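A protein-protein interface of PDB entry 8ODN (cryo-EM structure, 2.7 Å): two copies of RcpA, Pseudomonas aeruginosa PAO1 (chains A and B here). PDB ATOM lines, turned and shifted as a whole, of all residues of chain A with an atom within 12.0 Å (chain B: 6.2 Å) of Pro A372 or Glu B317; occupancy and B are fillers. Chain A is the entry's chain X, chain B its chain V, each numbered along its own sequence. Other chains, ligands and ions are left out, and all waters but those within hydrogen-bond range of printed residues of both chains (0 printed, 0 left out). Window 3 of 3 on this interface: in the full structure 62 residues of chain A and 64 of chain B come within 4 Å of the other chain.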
ATOM      1  N   PRO A 131      10.388   2.081  14.649  1.00  0.00           N
ATOM      2  CA  PRO A 131      11.209   3.057  13.932  1.00  0.00           C
ATOM      3  C   PRO A 131      10.393   3.971  13.026  1.00  0.00           C
ATOM      4  O   PRO A 131       9.401   3.538  12.441  1.00  0.00           O
ATOM      5  CB  PRO A 131      12.160   2.179  13.105  1.00  0.00           C
ATOM      6  CG  PRO A 131      11.939   0.745  13.580  1.00  0.00           C
ATOM      7  CD  PRO A 131      11.102   0.810  14.815  1.00  0.00           C
ATOM      8  N   ASN A 132      10.819   5.231  12.917  1.00  0.00           N
ATOM      9  CA  ASN A 132      10.137   6.223  12.094  1.00  0.00           C
ATOM     10  C   ASN A 132      11.042   6.759  10.989  1.00  0.00           C
ATOM     11  O   ASN A 132      10.747   7.806  10.405  1.00  0.00           O
ATOM     12  CB  ASN A 132       9.627   7.372  12.967  1.00  0.00           C
ATOM     13  CG  ASN A 132       8.609   8.238  12.254  1.00  0.00           C
ATOM     14  OD1 ASN A 132       7.928   7.787  11.334  1.00  0.00           O
ATOM     15  ND2 ASN A 132       8.500   9.491  12.678  1.00  0.00           N
ATOM     16  N   GLN A 133      12.136   6.064  10.693  1.00  0.00           N
ATOM     17  CA  GLN A 133      13.093   6.494   9.686  1.00  0.00           C
ATOM     18  C   GLN A 133      13.303   5.374   8.679  1.00  0.00           C
ATOM     19  O   GLN A 133      13.371   4.198   9.049  1.00  0.00           O
ATOM     20  CB  GLN A 133      14.418   6.896  10.333  1.00  0.00           C
ATOM     21  CG  GLN A 133      14.324   8.182  11.133  1.00  0.00           C
ATOM     22  CD  GLN A 133      15.311   8.236  12.275  1.00  0.00           C
ATOM     23  OE1 GLN A 133      15.023   7.789  13.383  1.00  0.00           O
ATOM     24  NE2 GLN A 133      16.482   8.795  12.012  1.00  0.00           N
ATOM     25  N   VAL A 134      13.409   5.749   7.407  1.00  0.00           N
ATOM     26  CA  VAL A 134      13.378   4.809   6.294  1.00  0.00           C
ATOM     27  C   VAL A 134      14.671   4.933   5.503  1.00  0.00           C
ATOM     28  O   VAL A 134      15.096   6.044   5.165  1.00  0.00           O
ATOM     29  CB  VAL A 134      12.164   5.058   5.382  1.00  0.00           C
ATOM     30  CG1 VAL A 134      12.102   4.019   4.275  1.00  0.00           C
ATOM     31  CG2 VAL A 134      10.882   5.057   6.190  1.00  0.00           C
ATOM     32  N   GLN A 135      15.289   3.794   5.210  1.00  0.00           N
ATOM     33  CA  GLN A 135      16.396   3.704   4.269  1.00  0.00           C
ATOM     34  C   GLN A 135      15.875   3.063   2.991  1.00  0.00           C
ATOM     35  O   GLN A 135      15.337   1.952   3.027  1.00  0.00           O
ATOM     36  CB  GLN A 135      17.551   2.889   4.850  1.00  0.00           C
ATOM     37  CG  GLN A 135      18.758   2.795   3.935  1.00  0.00           C
ATOM     38  CD  GLN A 135      19.848   1.908   4.493  1.00  0.00           C
ATOM     39  OE1 GLN A 135      19.612   1.107   5.397  1.00  0.00           O
ATOM     40  NE2 GLN A 135      21.053   2.046   3.958  1.00  0.00           N
ATOM     41  N   VAL A 225      18.775   7.809   3.343  1.00  0.00           N
ATOM     42  CA  VAL A 225      17.990   7.726   4.568  1.00  0.00           C
ATOM     43  C   VAL A 225      17.241   9.035   4.756  1.00  0.00           C
ATOM     44  O   VAL A 225      17.741  10.114   4.425  1.00  0.00           O
ATOM     45  CB  VAL A 225      18.870   7.430   5.800  1.00  0.00           C
ATOM     46  CG1 VAL A 225      18.014   7.317   7.046  1.00  0.00           C
ATOM     47  CG2 VAL A 225      19.683   6.167   5.593  1.00  0.00           C
ATOM     48  N   ALA A 226      16.027   8.934   5.293  1.00  0.00           N
ATOM     49  CA  ALA A 226      15.220  10.115   5.552  1.00  0.00           C
ATOM     50  C   ALA A 226      14.165   9.777   6.592  1.00  0.00           C
ATOM     51  O   ALA A 226      13.702   8.638   6.681  1.00  0.00           O
ATOM     52  CB  ALA A 226      14.557  10.632   4.274  1.00  0.00           C
ATOM     53  N   MET A 227      13.796  10.783   7.379  1.00  0.00           N
ATOM     54  CA  MET A 227      12.736  10.622   8.357  1.00  0.00           C
ATOM     55  C   MET A 227      11.377  10.607   7.663  1.00  0.00           C
ATOM     56  O   MET A 227      11.205  11.135   6.562  1.00  0.00           O
ATOM     57  CB  MET A 227      12.791  11.743   9.395  1.00  0.00           C
ATOM     58  CG  MET A 227      11.830  11.563  10.556  1.00  0.00           C
ATOM     59  SD  MET A 227      12.008  12.815  11.838  1.00  0.00           S
ATOM     60  CE  MET A 227      10.756  12.270  12.997  1.00  0.00           C
ATOM     61  N   SER A 228      10.404   9.989   8.327  1.00  0.00           N
ATOM     62  CA  SER A 228       9.070   9.869   7.756  1.00  0.00           C
ATOM     63  C   SER A 228       8.485  11.244   7.467  1.00  0.00           C
ATOM     64  O   SER A 228       8.496  12.133   8.324  1.00  0.00           O
ATOM     65  CB  SER A 228       8.161   9.099   8.711  1.00  0.00           C
ATOM     66  OG  SER A 228       6.831   9.054   8.226  1.00  0.00           O
ATOM     67  N   HIS A 368      13.583   0.006   3.779  1.00  0.00           N
ATOM     68  CA  HIS A 368      13.840  -0.654   5.052  1.00  0.00           C
ATOM     69  C   HIS A 368      13.639   0.335   6.189  1.00  0.00           C
ATOM     70  O   HIS A 368      14.031   1.500   6.087  1.00  0.00           O
ATOM     71  CB  HIS A 368      15.263  -1.215   5.123  1.00  0.00           C
ATOM     72  CG  HIS A 368      15.569  -2.241   4.080  1.00  0.00           C
ATOM     73  ND1 HIS A 368      15.363  -3.589   4.279  1.00  0.00           N
ATOM     74  CD2 HIS A 368      16.083  -2.119   2.833  1.00  0.00           C
ATOM     75  CE1 HIS A 368      15.729  -4.252   3.197  1.00  0.00           C
ATOM     76  NE2 HIS A 368      16.169  -3.384   2.305  1.00  0.00           N
ATOM     77  N   LEU A 369      13.025  -0.134   7.272  1.00  0.00           N
ATOM     78  CA  LEU A 369      12.970   0.637   8.505  1.00  0.00           C
ATOM     79  C   LEU A 369      14.249   0.400   9.298  1.00  0.00           C
ATOM     80  O   LEU A 369      14.645  -0.748   9.522  1.00  0.00           O
ATOM     81  CB  LEU A 369      11.746   0.242   9.329  1.00  0.00           C
ATOM     82  CG  LEU A 369      10.392   0.402   8.636  1.00  0.00           C
ATOM     83  CD1 LEU A 369       9.260   0.048   9.585  1.00  0.00           C
ATOM     84  CD2 LEU A 369      10.221   1.809   8.102  1.00  0.00           C
ATOM     85  N   VAL A 370      14.894   1.486   9.726  1.00  0.00           N
ATOM     86  CA  VAL A 370      16.225   1.424  10.317  1.00  0.00           C
ATOM     87  C   VAL A 370      16.259   2.271  11.582  1.00  0.00           C
ATOM     88  O   VAL A 370      15.360   3.068  11.854  1.00  0.00           O
ATOM     89  CB  VAL A 370      17.317   1.895   9.333  1.00  0.00           C
ATOM     90  CG1 VAL A 370      17.393   0.958   8.150  1.00  0.00           C
ATOM     91  CG2 VAL A 370      17.043   3.316   8.871  1.00  0.00           C
ATOM     92  N   GLN A 371      17.321   2.083  12.354  1.00  0.00           N
ATOM     93  CA  GLN A 371      17.581   2.836  13.568  1.00  0.00           C
ATOM     94  C   GLN A 371      19.038   3.268  13.568  1.00  0.00           C
ATOM     95  O   GLN A 371      19.878   2.637  12.917  1.00  0.00           O
ATOM     96  CB  GLN A 371      17.279   2.010  14.825  1.00  0.00           C
ATOM     97  CG  GLN A 371      15.801   1.876  15.133  1.00  0.00           C
ATOM     98  CD  GLN A 371      15.541   1.076  16.391  1.00  0.00           C
ATOM     99  OE1 GLN A 371      14.980   1.588  17.360  1.00  0.00           O
ATOM    100  NE2 GLN A 371      15.944  -0.188  16.383  1.00  0.00           N
ATOM    101  N   PRO A 372      19.369   4.339  14.288  1.00  0.00           N
ATOM    102  CA  PRO A 372      20.753   4.828  14.276  1.00  0.00           C
ATOM    103  C   PRO A 372      21.716   3.822  14.885  1.00  0.00           C
ATOM    104  O   PRO A 372      21.356   3.026  15.754  1.00  0.00           O
ATOM    105  CB  PRO A 372      20.688   6.109  15.117  1.00  0.00           C
ATOM    106  CG  PRO A 372      19.243   6.447  15.234  1.00  0.00           C
ATOM    107  CD  PRO A 372      18.505   5.161  15.148  1.00  0.00           C
ATOM    108  N   LEU A 373      22.959   3.869  14.413  1.00  0.00           N
ATOM    109  CA  LEU A 373      24.017   3.086  15.033  1.00  0.00           C
ATOM    110  C   LEU A 373      24.217   3.530  16.476  1.00  0.00           C
ATOM    111  O   LEU A 373      24.086   4.712  16.804  1.00  0.00           O
ATOM    112  CB  LEU A 373      25.322   3.242  14.252  1.00  0.00           C
ATOM    113  CG  LEU A 373      25.283   2.856  12.774  1.00  0.00           C
ATOM    114  CD1 LEU A 373      26.601   3.198  12.105  1.00  0.00           C
ATOM    115  CD2 LEU A 373      24.970   1.383  12.615  1.00  0.00           C
ATOM    116  N   ALA A 374      24.538   2.574  17.342  1.00  0.00           N
ATOM    117  CA  ALA A 374      24.705   2.879  18.753  1.00  0.00           C
ATOM    118  C   ALA A 374      25.940   3.748  18.973  1.00  0.00           C
ATOM    119  O   ALA A 374      26.844   3.820  18.137  1.00  0.00           O
ATOM    120  CB  ALA A 374      24.812   1.593  19.570  1.00  0.00           C
ATOM    121  N   ALA A 375      25.965   4.419  20.128  1.00  0.00           N
ATOM    122  CA  ALA A 375      27.053   5.345  20.423  1.00  0.00           C
ATOM    123  C   ALA A 375      28.406   4.648  20.425  1.00  0.00           C
ATOM    124  O   ALA A 375      29.422   5.269  20.091  1.00  0.00           O
ATOM    125  CB  ALA A 375      26.806   6.023  21.771  1.00  0.00           C
ATOM    126  N   ASP A 376      28.445   3.372  20.796  1.00  0.00           N
ATOM    127  CA  ASP A 376      29.688   2.615  20.856  1.00  0.00           C
ATOM    128  C   ASP A 376      29.978   1.844  19.576  1.00  0.00           C
ATOM    129  O   ASP A 376      30.980   1.126  19.516  1.00  0.00           O
ATOM    130  CB  ASP A 376      29.651   1.642  22.038  1.00  0.00           C
ATOM    131  CG  ASP A 376      28.550   0.605  21.908  1.00  0.00           C
ATOM    132  OD1 ASP A 376      27.727   0.722  20.977  1.00  0.00           O
ATOM    133  OD2 ASP A 376      28.511  -0.329  22.735  1.00  0.00           O
ATOM    134  N   ALA A 377      29.130   1.969  18.559  1.00  0.00           N
ATOM    135  CA  ALA A 377      29.279   1.165  17.356  1.00  0.00           C
ATOM    136  C   ALA A 377      30.511   1.582  16.565  1.00  0.00           C
ATOM    137  O   ALA A 377      30.851   2.766  16.487  1.00  0.00           O
ATOM    138  CB  ALA A 377      28.036   1.293  16.478  1.00  0.00           C
ATOM    139  N   GLN A 378      31.182   0.596  15.978  1.00  0.00           N
ATOM    140  CA  GLN A 378      32.237   0.865  15.014  1.00  0.00           C
ATOM    141  C   GLN A 378      31.603   1.231  13.679  1.00  0.00           C
ATOM    142  O   GLN A 378      30.760   0.494  13.159  1.00  0.00           O
ATOM    143  CB  GLN A 378      33.146  -0.354  14.858  1.00  0.00           C
ATOM    144  CG  GLN A 378      34.346  -0.128  13.952  1.00  0.00           C
ATOM    145  CD  GLN A 378      34.642  -1.328  13.076  1.00  0.00           C
ATOM    146  OE1 GLN A 378      35.253  -2.300  13.518  1.00  0.00           O
ATOM    147  NE2 GLN A 378      34.203  -1.268  11.824  1.00  0.00           N
ATOM    148  N   LEU A 379      32.008   2.371  13.129  1.00  0.00           N
ATOM    149  CA  LEU A 379      31.371   2.877  11.928  1.00  0.00           C
ATOM    150  C   LEU A 379      31.688   1.985  10.727  1.00  0.00           C
ATOM    151  O   LEU A 379      32.755   1.368  10.666  1.00  0.00           O
ATOM    152  CB  LEU A 379      31.835   4.301  11.638  1.00  0.00           C
ATOM    153  CG  LEU A 379      31.481   5.366  12.676  1.00  0.00           C
ATOM    154  CD1 LEU A 379      32.127   6.691  12.303  1.00  0.00           C
ATOM    155  CD2 LEU A 379      29.974   5.514  12.798  1.00  0.00           C
ATOM    156  N   PRO A 380      30.775   1.896   9.759  1.00  0.00           N
ATOM    157  CA  PRO A 380      31.127   1.275   8.480  1.00  0.00           C
ATOM    158  C   PRO A 380      32.229   2.065   7.793  1.00  0.00           C
ATOM    159  O   PRO A 380      32.334   3.283   7.943  1.00  0.00           O
ATOM    160  CB  PRO A 380      29.817   1.320   7.686  1.00  0.00           C
ATOM    161  CG  PRO A 380      28.743   1.458   8.715  1.00  0.00           C
ATOM    162  CD  PRO A 380      29.347   2.250   9.828  1.00  0.00           C
ATOM    163  N   ARG B 274      17.177  13.916  22.295  1.00  0.00           N
ATOM    164  CA  ARG B 274      17.549  13.454  20.968  1.00  0.00           C
ATOM    165  C   ARG B 274      17.735  14.644  20.036  1.00  0.00           C
ATOM    166  O   ARG B 274      17.119  15.699  20.209  1.00  0.00           O
ATOM    167  CB  ARG B 274      16.491  12.506  20.403  1.00  0.00           C
ATOM    168  CG  ARG B 274      16.397  11.180  21.133  1.00  0.00           C
ATOM    169  CD  ARG B 274      16.251  10.025  20.157  1.00  0.00           C
ATOM    170  NE  ARG B 274      15.112  10.199  19.263  1.00  0.00           N
ATOM    171  CZ  ARG B 274      14.930   9.515  18.142  1.00  0.00           C
ATOM    172  NH1 ARG B 274      15.805   8.612  17.731  1.00  0.00           N
ATOM    173  NH2 ARG B 274      13.844   9.747  17.410  1.00  0.00           N
ATOM    174  N   MET B 312      16.901  11.981  12.798  1.00  0.00           N
ATOM    175  CA  MET B 312      16.910  12.134  14.247  1.00  0.00           C
ATOM    176  C   MET B 312      17.872  11.118  14.842  1.00  0.00           C
ATOM    177  O   MET B 312      17.823   9.935  14.492  1.00  0.00           O
ATOM    178  CB  MET B 312      15.511  11.943  14.836  1.00  0.00           C
ATOM    179  CG  MET B 312      14.583  13.120  14.619  1.00  0.00           C
ATOM    180  SD  MET B 312      12.966  12.885  15.378  1.00  0.00           S
ATOM    181  CE  MET B 312      12.223  14.483  15.071  1.00  0.00           C
ATOM    182  N   LEU B 313      18.738  11.579  15.742  1.00  0.00           N
ATOM    183  CA  LEU B 313      19.701  10.715  16.406  1.00  0.00           C
ATOM    184  C   LEU B 313      19.827  11.131  17.862  1.00  0.00           C
ATOM    185  O   LEU B 313      19.471  12.247  18.245  1.00  0.00           O
ATOM    186  CB  LEU B 313      21.085  10.772  15.745  1.00  0.00           C
ATOM    187  CG  LEU B 313      21.180  10.590  14.233  1.00  0.00           C
ATOM    188  CD1 LEU B 313      20.984  11.911  13.519  1.00  0.00           C
ATOM    189  CD2 LEU B 313      22.517   9.985  13.866  1.00  0.00           C
ATOM    190  N   ALA B 314      20.340  10.214  18.674  1.00  0.00           N
ATOM    191  CA  ALA B 314      20.693  10.517  20.050  1.00  0.00           C
ATOM    192  C   ALA B 314      22.157  10.936  20.126  1.00  0.00           C
ATOM    193  O   ALA B 314      22.952  10.674  19.220  1.00  0.00           O
ATOM    194  CB  ALA B 314      20.438   9.315  20.957  1.00  0.00           C
ATOM    195  N   ASP B 315      22.504  11.605  21.221  1.00  0.00           N
ATOM    196  CA  ASP B 315      23.863  12.095  21.409  1.00  0.00           C
ATOM    197  C   ASP B 315      24.878  10.984  21.186  1.00  0.00           C
ATOM    198  O   ASP B 315      24.899   9.990  21.916  1.00  0.00           O
ATOM    199  CB  ASP B 315      24.015  12.679  22.815  1.00  0.00           C
ATOM    200  CG  ASP B 315      25.444  13.070  23.132  1.00  0.00           C
ATOM    201  OD1 ASP B 315      25.994  13.942  22.429  1.00  0.00           O
ATOM    202  OD2 ASP B 315      26.018  12.505  24.086  1.00  0.00           O
ATOM    203  N   GLY B 316      25.723  11.161  20.170  1.00  0.00           N
ATOM    204  CA  GLY B 316      26.774  10.222  19.859  1.00  0.00           C
ATOM    205  C   GLY B 316      26.422   9.175  18.823  1.00  0.00           C
ATOM    206  O   GLY B 316      27.330   8.533  18.282  1.00  0.00           O
ATOM    207  N   GLU B 317      25.140   8.981  18.525  1.00  0.00           N
ATOM    208  CA  GLU B 317      24.756   7.998  17.526  1.00  0.00           C
ATOM    209  C   GLU B 317      25.113   8.501  16.128  1.00  0.00           C
ATOM    210  O   GLU B 317      25.419   9.678  15.917  1.00  0.00           O
ATOM    211  CB  GLU B 317      23.264   7.683  17.627  1.00  0.00           C
ATOM    212  CG  GLU B 317      22.883   6.927  18.890  1.00  0.00           C
ATOM    213  CD  GLU B 317      21.414   6.557  18.937  1.00  0.00           C
ATOM    214  OE1 GLU B 317      20.629   7.119  18.146  1.00  0.00           O
ATOM    215  OE2 GLU B 317      21.044   5.702  19.767  1.00  0.00           O
ATOM    216  N   SER B 318      25.072   7.587  15.160  1.00  0.00           N
ATOM    217  CA  SER B 318      25.539   7.872  13.813  1.00  0.00           C
ATOM    218  C   SER B 318      24.597   7.257  12.789  1.00  0.00           C
ATOM    219  O   SER B 318      23.853   6.316  13.078  1.00  0.00           O
ATOM    220  CB  SER B 318      26.960   7.344  13.593  1.00  0.00           C
ATOM    221  OG  SER B 318      27.398   7.600  12.271  1.00  0.00           O
ATOM    222  N   PHE B 319      24.638   7.814  11.580  1.00  0.00           N
ATOM    223  CA  PHE B 319      23.892   7.299  10.443  1.00  0.00           C
ATOM    224  C   PHE B 319      24.784   7.295   9.213  1.00  0.00           C
ATOM    225  O   PHE B 319      25.641   8.165   9.049  1.00  0.00           O
ATOM    226  CB  PHE B 319      22.652   8.147  10.132  1.00  0.00           C
ATOM    227  CG  PHE B 319      21.364   7.541  10.592  1.00  0.00           C
ATOM    228  CD1 PHE B 319      20.967   6.296  10.138  1.00  0.00           C
ATOM    229  CD2 PHE B 319      20.534   8.229  11.451  1.00  0.00           C
ATOM    230  CE1 PHE B 319      19.778   5.744  10.554  1.00  0.00           C
ATOM    231  CE2 PHE B 319      19.345   7.684  11.867  1.00  0.00           C
ATOM    232  CZ  PHE B 319      18.964   6.439  11.417  1.00  0.00           C
ATOM    233  N   VAL B 365      27.047  10.980   9.474  1.00  0.00           N
ATOM    234  CA  VAL B 365      26.812  12.125  10.341  1.00  0.00           C
ATOM    235  C   VAL B 365      26.845  11.656  11.787  1.00  0.00           C
ATOM    236  O   VAL B 365      26.424  10.540  12.109  1.00  0.00           O
ATOM    237  CB  VAL B 365      25.470  12.815  10.016  1.00  0.00           C
ATOM    238  CG1 VAL B 365      24.304  11.902  10.346  1.00  0.00           C
ATOM    239  CG2 VAL B 365      25.352  14.125  10.762  1.00  0.00           C
ATOM    240  N   THR B 366      27.351  12.522  12.665  1.00  0.00           N
ATOM    241  CA  THR B 366      27.466  12.195  14.080  1.00  0.00           C
ATOM    242  C   THR B 366      27.341  13.457  14.926  1.00  0.00           C
ATOM    243  O   THR B 366      28.281  14.261  14.983  1.00  0.00           O
ATOM    244  CB  THR B 366      28.799  11.507  14.372  1.00  0.00           C
ATOM    245  OG1 THR B 366      29.009  10.444  13.435  1.00  0.00           O
ATOM    246  CG2 THR B 366      28.806  10.941  15.779  1.00  0.00           C
ATOM    247  N   PRO B 367      26.208  13.670  15.598  1.00  0.00           N
ATOM    248  CA  PRO B 367      26.065  14.850  16.455  1.00  0.00           C
ATOM    249  C   PRO B 367      26.485  14.595  17.895  1.00  0.00           C
ATOM    250  O   PRO B 367      26.236  13.534  18.468  1.00  0.00           O
ATOM    251  CB  PRO B 367      24.561  15.141  16.370  1.00  0.00           C
ATOM    252  CG  PRO B 367      23.950  13.801  16.207  1.00  0.00           C
ATOM    253  CD  PRO B 367      24.926  12.969  15.419  1.00  0.00           C
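N of Ala B314 sits at hydrogen-bond distance from OE1 of Glu B317.
The backbone NH (N) of Gly B316 lies within hydrogen-bond range of the backbone carbonyl oxygen (O) of Pro B367.
The backbone carbonyl oxygen of Val B365 lies within hydrogen-bond range of the side-chain hydroxyl of Ser B318 (3.1 Å).
The side-chain hydroxyl (OG) of Ser B318 is in hydrogen-bond range of the side-chain hydroxyl (OG1) of Thr B366, 3.5 Å away.
O of Phe B319 lies within hydrogen-bond range of N of Val B365 (3.2 Å).
O of Gln A133 lies within hydrogen-bond range of N of Val A370, 3.2 Å away.
No position is printed for both chains.
Of the 12 pairs that touch across the chains among the printed residues, none has its exchanged pair printed and touching as well.
Among the printed residues, pairs that only touch across the chains: Gln A133 with Phe B319, Gln A371 with Phe B319, Pro A372 with Met B312, Pro A372 with Glu B317, Pro A372 with Ser B318, Pro A372 with Phe B319, Leu A373 with Glu B317, Ala A375 with Gly B316 and Leu A379 with Ser B318.
Of the printed residues of chain B, Gln A133 touches Met B312 (3.0 Å) and Phe B319 (3.1 Å).
Of the printed residues of chain B, Gln A371 touches Phe B319.
Pro A372 touches four residues of chain B.
Of the printed residues of chain B, Leu A373 touches Glu B317 and Ser B318.
Asp A376 touches none of the printed residues of chain B.
Of the printed residues of chain B, Leu A379 touches Ser B318 (3.4 Å).
Of the printed residues of chain A, Met B312 touches Gln A133, Met A227 and Pro A372.
No residue of chain A comes within 4 Å of Ala B314.
Gly B316 touches just one residue of chain A: Ala A375 (3.9 Å).
Of the printed residues of chain A, Glu B317 touches Pro A372 and Leu A373.
Of chain A, only Pro A372, Leu A373 and Leu A379 come within 4 Å of Ser B318.
No residue of chain A comes within 4 Å of Val B365.
No residue of chain A comes within 4 Å of Pro B367.
The nearest residue of chain B that does not touch Pro A372 is Leu B313 (4.4 Å).
The nearest residue of chain A that does not touch Glu B317 is Ala A375 (4.2 Å).
Hydrophobic or aromatic side chains of chain B that line the printed part of chain A: Met B312 and Phe B319.
Printed residues of chain A that touch a printed residue of chain B: Gln A133, Met A227, Gln A371, Pro A372, Leu A373, Ala A375 and Leu A379.
O of Met B312 is in hydrogen-bond range of NE2 of Gln A133, 3.0 Å away.
The backbone carbonyl oxygen (O) of Ser B318 is in hydrogen-bond range of the backbone NH (N) of Leu A373, at 2.9 Å.
SD of Met A227 lies close to SD of Met B312 (3.7 Å).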
